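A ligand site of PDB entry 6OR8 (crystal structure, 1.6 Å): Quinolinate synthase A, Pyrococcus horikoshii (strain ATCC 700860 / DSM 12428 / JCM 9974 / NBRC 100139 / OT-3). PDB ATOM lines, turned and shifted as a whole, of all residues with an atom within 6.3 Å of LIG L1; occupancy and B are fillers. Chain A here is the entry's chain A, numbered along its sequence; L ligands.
FE3 of LIG L1 is bound by O2 of LG2 L2 (2.3 Å).
The side-chain sulfur (SG) of Cys 170 is bound to an iron atom (FE4) of LIG L1, 2.3 Å away.
The side-chain sulfur (SG) of Cys 83 is bound to an iron atom (FE2) of LIG L1 (2.3 Å).
SG of Cys 256 is bound to FE1 of LIG L1 (2.4 Å).
S3 of LIG L1 lies close to N of Ala 84, 3.7 Å away.
ND2 of Asn 111 is in hydrogen-bond range of O5 of LG2 L2, at 3.0 Å.
NE2 of His 21 sits at hydrogen-bond distance from O4 of LG2 L2, 2.8 Å away.
The side-chain sulfur (SG) of Cys 170 lies close to the side-chain carboxylate (OE1) of Glu 198, at 3.7 Å.
The side-chain sulfur (SG) of Cys 170 sits close to the backbone NH (N) of Val 172.
A ring nitrogen (ND1) of His 173 lies close to the side-chain sulfur of Cys 170.
The side-chain sulfur (SG) of Cys 83 sits close to the backbone NH (N) of Met 85 (3.7 Å).
N of Met 259 sits close to SG of Cys 256.
The backbone NH of Cys 256 sits at hydrogen-bond distance from the side-chain carboxylate of Glu 231, at 2.8 Å.
OE1 of Glu 198 lies within hydrogen-bond range of ND1 of His 173.
A ring nitrogen (ND1) of His 21 is in hydrogen-bond range of the backbone NH (N) of Tyr 23 (2.9 Å).
A sulfur (S1) of LIG L1 sits close to the side-chain carboxylate (OE1) of Glu 198 (3.7 Å).
Merely in contact with LIG L1: Tyr 23 (3.9 Å), Val 58 (3.9 Å), Met 85 (3.9 Å) and Val 172 (3.8 Å).
The nearest printed residue that does not touch LIG L1 is Tyr 171 (4.1 Å).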
ATOM      1  N   HIS A  21      -8.218  16.676   6.409  1.00  0.00           N
ATOM      2  CA  HIS A  21      -7.774  16.828   5.039  1.00  0.00           C
ATOM      3  C   HIS A  21      -6.241  16.920   4.982  1.00  0.00           C
ATOM      4  O   HIS A  21      -5.572  17.272   5.963  1.00  0.00           O
ATOM      5  CB  HIS A  21      -8.405  18.081   4.406  1.00  0.00           C
ATOM      6  CG  HIS A  21      -8.129  18.208   2.944  1.00  0.00           C
ATOM      7  ND1 HIS A  21      -7.054  18.914   2.436  1.00  0.00           N
ATOM      8  CD2 HIS A  21      -8.770  17.683   1.876  1.00  0.00           C
ATOM      9  CE1 HIS A  21      -7.051  18.816   1.120  1.00  0.00           C
ATOM     10  NE2 HIS A  21      -8.081  18.068   0.757  1.00  0.00           N
ATOM     11  N   TYR A  23      -4.431  19.100   3.682  1.00  0.00           N
ATOM     12  CA  TYR A  23      -3.905  20.438   3.922  1.00  0.00           C
ATOM     13  C   TYR A  23      -3.955  20.858   5.374  1.00  0.00           C
ATOM     14  O   TYR A  23      -3.672  22.019   5.678  1.00  0.00           O
ATOM     15  CB  TYR A  23      -4.670  21.494   3.117  1.00  0.00           C
ATOM     16  CG  TYR A  23      -4.656  21.334   1.634  1.00  0.00           C
ATOM     17  CD1 TYR A  23      -3.702  20.533   0.984  1.00  0.00           C
ATOM     18  CD2 TYR A  23      -5.611  21.979   0.866  1.00  0.00           C
ATOM     19  CE1 TYR A  23      -3.713  20.415  -0.409  1.00  0.00           C
ATOM     20  CE2 TYR A  23      -5.627  21.870  -0.505  1.00  0.00           C
ATOM     21  CZ  TYR A  23      -4.688  21.086  -1.138  1.00  0.00           C
ATOM     22  OH  TYR A  23      -4.750  20.988  -2.503  1.00  0.00           O
ATOM     23  N   VAL A  58     -12.842  21.977   5.386  1.00  0.00           N
ATOM     24  CA  VAL A  58     -13.686  23.117   5.079  1.00  0.00           C
ATOM     25  C   VAL A  58     -15.144  22.684   4.868  1.00  0.00           C
ATOM     26  O   VAL A  58     -15.475  21.493   4.812  1.00  0.00           O
ATOM     27  CB  VAL A  58     -13.148  23.917   3.869  1.00  0.00           C
ATOM     28  CG1 VAL A  58     -11.769  24.491   4.224  1.00  0.00           C
ATOM     29  CG2 VAL A  58     -13.103  23.020   2.620  1.00  0.00           C
ATOM     30  N   PHE A  60     -17.620  22.492   2.581  1.00  0.00           N
ATOM     31  CA  PHE A  60     -18.213  21.542   1.639  1.00  0.00           C
ATOM     32  C   PHE A  60     -17.771  20.121   1.922  1.00  0.00           C
ATOM     33  O   PHE A  60     -18.482  19.173   1.574  1.00  0.00           O
ATOM     34  CB  PHE A  60     -17.878  21.914   0.174  1.00  0.00           C
ATOM     35  CG  PHE A  60     -16.469  21.547  -0.284  1.00  0.00           C
ATOM     36  CD1 PHE A  60     -16.132  20.241  -0.640  1.00  0.00           C
ATOM     37  CD2 PHE A  60     -15.499  22.521  -0.406  1.00  0.00           C
ATOM     38  CE1 PHE A  60     -14.845  19.912  -1.045  1.00  0.00           C
ATOM     39  CE2 PHE A  60     -14.218  22.212  -0.824  1.00  0.00           C
ATOM     40  CZ  PHE A  60     -13.885  20.914  -1.144  1.00  0.00           C
ATOM     41  N   MET A  61     -16.589  19.949   2.527  1.00  0.00           N
ATOM     42  CA  MET A  61     -16.112  18.606   2.800  1.00  0.00           C
ATOM     43  C   MET A  61     -16.914  17.977   3.943  1.00  0.00           C
ATOM     44  O   MET A  61     -17.246  16.795   3.902  1.00  0.00           O
ATOM     45  CB  MET A  61     -14.623  18.631   3.140  1.00  0.00           C
ATOM     46  CG  MET A  61     -13.791  19.448   2.205  1.00  0.00           C
ATOM     47  SD  MET A  61     -12.047  19.349   2.664  1.00  0.00           S
ATOM     48  CE  MET A  61     -11.260  19.981   1.194  1.00  0.00           C
ATOM     49  N   THR A  82     -13.939  27.665   5.276  1.00  0.00           N
ATOM     50  CA  THR A  82     -14.749  27.737   4.060  1.00  0.00           C
ATOM     51  C   THR A  82     -13.873  27.663   2.811  1.00  0.00           C
ATOM     52  O   THR A  82     -12.682  27.997   2.843  1.00  0.00           O
ATOM     53  CB  THR A  82     -15.560  29.043   4.011  1.00  0.00           C
ATOM     54  OG1 THR A  82     -14.640  30.138   3.948  1.00  0.00           O
ATOM     55  CG2 THR A  82     -16.443  29.178   5.241  1.00  0.00           C
ATOM     56  N   CYS A  83     -14.498  27.223   1.708  1.00  0.00           N
ATOM     57  CA  CYS A  83     -13.836  27.104   0.415  1.00  0.00           C
ATOM     58  C   CYS A  83     -14.246  28.245  -0.500  1.00  0.00           C
ATOM     59  O   CYS A  83     -15.433  28.365  -0.878  1.00  0.00           O
ATOM     60  CB  CYS A  83     -14.184  25.755  -0.249  1.00  0.00           C
ATOM     61  SG  CYS A  83     -13.520  25.553  -1.908  1.00  0.00           S
ATOM     62  N   ALA A  84     -13.278  29.089  -0.861  1.00  0.00           N
ATOM     63  CA  ALA A  84     -13.580  30.264  -1.676  1.00  0.00           C
ATOM     64  C   ALA A  84     -14.042  29.876  -3.065  1.00  0.00           C
ATOM     65  O   ALA A  84     -14.932  30.513  -3.634  1.00  0.00           O
ATOM     66  CB  ALA A  84     -12.349  31.171  -1.779  1.00  0.00           C
ATOM     67  N   MET A  85     -13.472  28.791  -3.612  1.00  0.00           N
ATOM     68  CA  MET A  85     -13.853  28.384  -4.955  1.00  0.00           C
ATOM     69  C   MET A  85     -15.269  27.818  -4.983  1.00  0.00           C
ATOM     70  O   MET A  85     -16.088  28.207  -5.832  1.00  0.00           O
ATOM     71  CB  MET A  85     -12.824  27.368  -5.499  1.00  0.00           C
ATOM     72  CG  MET A  85     -13.066  26.928  -6.933  1.00  0.00           C
ATOM     73  SD  MET A  85     -14.104  25.464  -6.999  1.00  0.00           S
ATOM     74  CE  MET A  85     -13.002  24.246  -6.272  1.00  0.00           C
ATOM     75  N   ALA A  86     -15.588  26.926  -4.040  1.00  0.00           N
ATOM     76  CA  ALA A  86     -16.906  26.293  -4.019  1.00  0.00           C
ATOM     77  C   ALA A  86     -17.994  27.337  -3.831  1.00  0.00           C
ATOM     78  O   ALA A  86     -19.074  27.232  -4.421  1.00  0.00           O
ATOM     79  CB  ALA A  86     -16.996  25.260  -2.904  1.00  0.00           C
ATOM     80  N   ASN A 111     -15.294  19.138  -5.158  1.00  0.00           N
ATOM     81  CA  ASN A 111     -15.081  20.390  -4.435  1.00  0.00           C
ATOM     82  C   ASN A 111     -16.202  21.354  -4.829  1.00  0.00           C
ATOM     83  O   ASN A 111     -16.071  22.192  -5.733  1.00  0.00           O
ATOM     84  CB  ASN A 111     -13.718  21.004  -4.756  1.00  0.00           C
ATOM     85  CG  ASN A 111     -12.555  20.073  -4.488  1.00  0.00           C
ATOM     86  OD1 ASN A 111     -12.711  18.863  -4.389  1.00  0.00           O
ATOM     87  ND2 ASN A 111     -11.355  20.659  -4.380  1.00  0.00           N
ATOM     88  N   ASP A 146     -14.830  25.017 -11.072  1.00  0.00           N
ATOM     89  CA  ASP A 146     -13.460  25.486 -11.312  1.00  0.00           C
ATOM     90  C   ASP A 146     -13.180  25.535 -12.798  1.00  0.00           C
ATOM     91  O   ASP A 146     -13.185  24.499 -13.465  1.00  0.00           O
ATOM     92  CB  ASP A 146     -12.456  24.579 -10.629  1.00  0.00           C
ATOM     93  CG  ASP A 146     -11.076  25.142 -10.668  1.00  0.00           C
ATOM     94  OD1 ASP A 146     -10.380  24.955 -11.681  1.00  0.00           O
ATOM     95  OD2 ASP A 146     -10.677  25.762  -9.664  1.00  0.00           O
ATOM     96  N   CYS A 170      -9.847  28.697  -7.763  1.00  0.00           N
ATOM     97  CA  CYS A 170      -9.301  28.634  -6.405  1.00  0.00           C
ATOM     98  C   CYS A 170      -8.121  29.584  -6.335  1.00  0.00           C
ATOM     99  O   CYS A 170      -7.139  29.391  -7.059  1.00  0.00           O
ATOM    100  CB  CYS A 170      -8.854  27.212  -6.079  1.00  0.00           C
ATOM    101  SG  CYS A 170      -7.742  27.132  -4.677  1.00  0.00           S
ATOM    102  N   TYR A 171      -8.199  30.595  -5.457  1.00  0.00           N
ATOM    103  CA  TYR A 171      -7.118  31.588  -5.366  1.00  0.00           C
ATOM    104  C   TYR A 171      -5.795  30.951  -4.927  1.00  0.00           C
ATOM    105  O   TYR A 171      -4.715  31.486  -5.246  1.00  0.00           O
ATOM    106  CB  TYR A 171      -7.485  32.708  -4.396  1.00  0.00           C
ATOM    107  CG  TYR A 171      -7.537  32.293  -2.928  1.00  0.00           C
ATOM    108  CD1 TYR A 171      -8.670  31.678  -2.411  1.00  0.00           C
ATOM    109  CD2 TYR A 171      -6.454  32.499  -2.079  1.00  0.00           C
ATOM    110  CE1 TYR A 171      -8.724  31.279  -1.057  1.00  0.00           C
ATOM    111  CE2 TYR A 171      -6.491  32.104  -0.748  1.00  0.00           C
ATOM    112  CZ  TYR A 171      -7.648  31.485  -0.249  1.00  0.00           C
ATOM    113  OH  TYR A 171      -7.720  31.075   1.064  1.00  0.00           O
ATOM    114  N   VAL A 172      -5.836  29.861  -4.177  1.00  0.00           N
ATOM    115  CA  VAL A 172      -4.598  29.219  -3.726  1.00  0.00           C
ATOM    116  C   VAL A 172      -3.827  28.677  -4.923  1.00  0.00           C
ATOM    117  O   VAL A 172      -2.601  28.850  -5.007  1.00  0.00           O
ATOM    118  CB  VAL A 172      -4.894  28.084  -2.722  1.00  0.00           C
ATOM    119  CG1 VAL A 172      -3.569  27.532  -2.152  1.00  0.00           C
ATOM    120  CG2 VAL A 172      -5.831  28.561  -1.611  1.00  0.00           C
ATOM    121  N   HIS A 173      -4.518  28.014  -5.837  1.00  0.00           N
ATOM    122  CA  HIS A 173      -3.821  27.415  -6.961  1.00  0.00           C
ATOM    123  C   HIS A 173      -3.635  28.375  -8.104  1.00  0.00           C
ATOM    124  O   HIS A 173      -2.718  28.205  -8.898  1.00  0.00           O
ATOM    125  CB  HIS A 173      -4.559  26.154  -7.448  1.00  0.00           C
ATOM    126  CG  HIS A 173      -4.513  25.047  -6.446  1.00  0.00           C
ATOM    127  ND1 HIS A 173      -5.460  24.919  -5.450  1.00  0.00           N
ATOM    128  CD2 HIS A 173      -3.614  24.054  -6.237  1.00  0.00           C
ATOM    129  CE1 HIS A 173      -5.154  23.879  -4.696  1.00  0.00           C
ATOM    130  NE2 HIS A 173      -4.038  23.330  -5.155  1.00  0.00           N
ATOM    131  N   GLU A 198      -6.270  22.516 -10.538  1.00  0.00           N
ATOM    132  CA  GLU A 198      -6.825  23.843 -10.330  1.00  0.00           C
ATOM    133  C   GLU A 198      -5.822  24.946 -10.682  1.00  0.00           C
ATOM    134  O   GLU A 198      -6.164  26.122 -10.592  1.00  0.00           O
ATOM    135  CB  GLU A 198      -7.290  23.988  -8.885  1.00  0.00           C
ATOM    136  CG  GLU A 198      -8.579  23.204  -8.565  1.00  0.00           C
ATOM    137  CD  GLU A 198      -8.860  23.125  -7.072  1.00  0.00           C
ATOM    138  OE1 GLU A 198      -8.142  23.779  -6.290  1.00  0.00           O
ATOM    139  OE2 GLU A 198      -9.773  22.401  -6.673  1.00  0.00           O
ATOM    140  N   GLU A 231      -1.387  23.439  -2.208  1.00  0.00           N
ATOM    141  CA  GLU A 231      -1.292  24.042  -0.893  1.00  0.00           C
ATOM    142  C   GLU A 231      -0.102  23.448  -0.142  1.00  0.00           C
ATOM    143  O   GLU A 231       0.107  22.234  -0.136  1.00  0.00           O
ATOM    144  CB  GLU A 231      -2.609  23.821  -0.140  1.00  0.00           C
ATOM    145  CG  GLU A 231      -3.000  24.937   0.811  1.00  0.00           C
ATOM    146  CD  GLU A 231      -2.485  24.764   2.229  1.00  0.00           C
ATOM    147  OE1 GLU A 231      -1.722  23.806   2.494  1.00  0.00           O
ATOM    148  OE2 GLU A 231      -2.813  25.622   3.094  1.00  0.00           O
ATOM    149  N   PHE A 255      -1.214  29.056   0.734  1.00  0.00           N
ATOM    150  CA  PHE A 255      -1.986  28.584   1.877  1.00  0.00           C
ATOM    151  C   PHE A 255      -3.481  28.756   1.642  1.00  0.00           C
ATOM    152  O   PHE A 255      -3.915  29.727   1.033  1.00  0.00           O
ATOM    153  CB  PHE A 255      -1.604  29.328   3.192  1.00  0.00           C
ATOM    154  CG  PHE A 255      -1.842  30.803   3.147  1.00  0.00           C
ATOM    155  CD1 PHE A 255      -3.072  31.337   3.492  1.00  0.00           C
ATOM    156  CD2 PHE A 255      -0.817  31.665   2.807  1.00  0.00           C
ATOM    157  CE1 PHE A 255      -3.286  32.715   3.448  1.00  0.00           C
ATOM    158  CE2 PHE A 255      -1.029  33.042   2.777  1.00  0.00           C
ATOM    159  CZ  PHE A 255      -2.261  33.567   3.094  1.00  0.00           C
ATOM    160  N   CYS A 256      -4.266  27.834   2.191  1.00  0.00           N
ATOM    161  CA  CYS A 256      -5.726  27.942   2.136  1.00  0.00           C
ATOM    162  C   CYS A 256      -6.213  28.495   3.472  1.00  0.00           C
ATOM    163  O   CYS A 256      -6.150  27.787   4.481  1.00  0.00           O
ATOM    164  CB  CYS A 256      -6.374  26.596   1.841  1.00  0.00           C
ATOM    165  SG  CYS A 256      -8.186  26.634   1.989  1.00  0.00           S
ATOM    166  N   ILE A 257      -6.708  29.740   3.485  1.00  0.00           N
ATOM    167  CA  ILE A 257      -7.108  30.363   4.747  1.00  0.00           C
ATOM    168  C   ILE A 257      -8.208  29.553   5.419  1.00  0.00           C
ATOM    169  O   ILE A 257      -8.242  29.437   6.649  1.00  0.00           O
ATOM    170  CB  ILE A 257      -7.563  31.810   4.509  1.00  0.00           C
ATOM    171  CG1 ILE A 257      -6.555  32.533   3.625  1.00  0.00           C
ATOM    172  CG2 ILE A 257      -7.710  32.554   5.818  1.00  0.00           C
ATOM    173  CD1 ILE A 257      -7.118  33.762   2.876  1.00  0.00           C
ATOM    174  N   GLY A 258      -9.109  28.949   4.635  1.00  0.00           N
ATOM    175  CA  GLY A 258     -10.197  28.175   5.235  1.00  0.00           C
ATOM    176  C   GLY A 258      -9.685  26.976   6.014  1.00  0.00           C
ATOM    177  O   GLY A 258     -10.184  26.676   7.102  1.00  0.00           O
ATOM    178  N   MET A 259      -8.679  26.281   5.460  1.00  0.00           N
ATOM    179  CA  MET A 259      -8.074  25.152   6.170  1.00  0.00           C
ATOM    180  C   MET A 259      -7.437  25.595   7.472  1.00  0.00           C
ATOM    181  O   MET A 259      -7.442  24.846   8.461  1.00  0.00           O
ATOM    182  CB  MET A 259      -7.013  24.492   5.310  1.00  0.00           C
ATOM    183  CG  MET A 259      -7.555  23.784   4.145  1.00  0.00           C
ATOM    184  SD  MET A 259      -8.412  22.253   4.646  1.00  0.00           S
ATOM    185  CE  MET A 259      -8.900  21.676   3.078  1.00  0.00           C
HETATM  186 FE1  LIG L   1      -8.993  25.906  -0.111  1.00  0.00          FE
HETATM  187 FE2  LIG L   1     -11.213  25.569  -1.637  1.00  0.00          FE
HETATM  188 FE3  LIG L   1      -9.216  23.807  -1.824  1.00  0.00          FE
HETATM  189 FE4  LIG L   1      -8.881  26.250  -2.859  1.00  0.00          FE
HETATM  190  S1  LIG L   1     -10.347  24.771  -3.502  1.00  0.00           S
HETATM  191  S2  LIG L   1      -7.479  25.167  -1.542  1.00  0.00           S
HETATM  192  S3  LIG L   1     -10.039  27.433  -1.372  1.00  0.00           S
HETATM  193  S4  LIG L   1     -10.473  24.277  -0.020  1.00  0.00           S
HETATM  194  O1  LG2 L   2      -8.118  22.121  -3.621  1.00  0.00           O
HETATM  195  C1  LG2 L   2      -8.297  21.294  -2.689  1.00  0.00           C
HETATM  196  O2  LG2 L   2      -9.053  21.535  -1.724  1.00  0.00           O
HETATM  197  C2  LG2 L   2      -7.566  19.975  -2.650  1.00  0.00           C
HETATM  198  C3  LG2 L   2      -8.470  18.833  -3.026  1.00  0.00           C
HETATM  199  C4  LG2 L   2      -7.604  17.604  -2.896  1.00  0.00           C
HETATM  200  O3  LG2 L   2      -7.119  17.179  -3.958  1.00  0.00           O
HETATM  201  O4  LG2 L   2      -7.361  17.114  -1.764  1.00  0.00           O
HETATM  202  O5  LG2 L   2      -8.837  19.048  -4.363  1.00  0.00           O
HETATM  203  N1  LG2 L   2      -9.651  18.704  -2.219  1.00  0.00           N
HETATM  204  C5  LG2 L   2     -10.030  17.321  -2.066  1.00  0.00           C
HETATM  205  O6  LG2 L   2     -10.854  17.176  -0.929  1.00  0.00           O
HETATM  206  C6  LG2 L   2     -10.733  16.751  -3.276  1.00  0.00           C
HETATM  207  C7  LG2 L   2      -9.935  16.470  -4.520  1.00  0.00           C
HETATM  208  O7  LG2 L   2     -10.416  17.122  -5.423  1.00  0.00           O
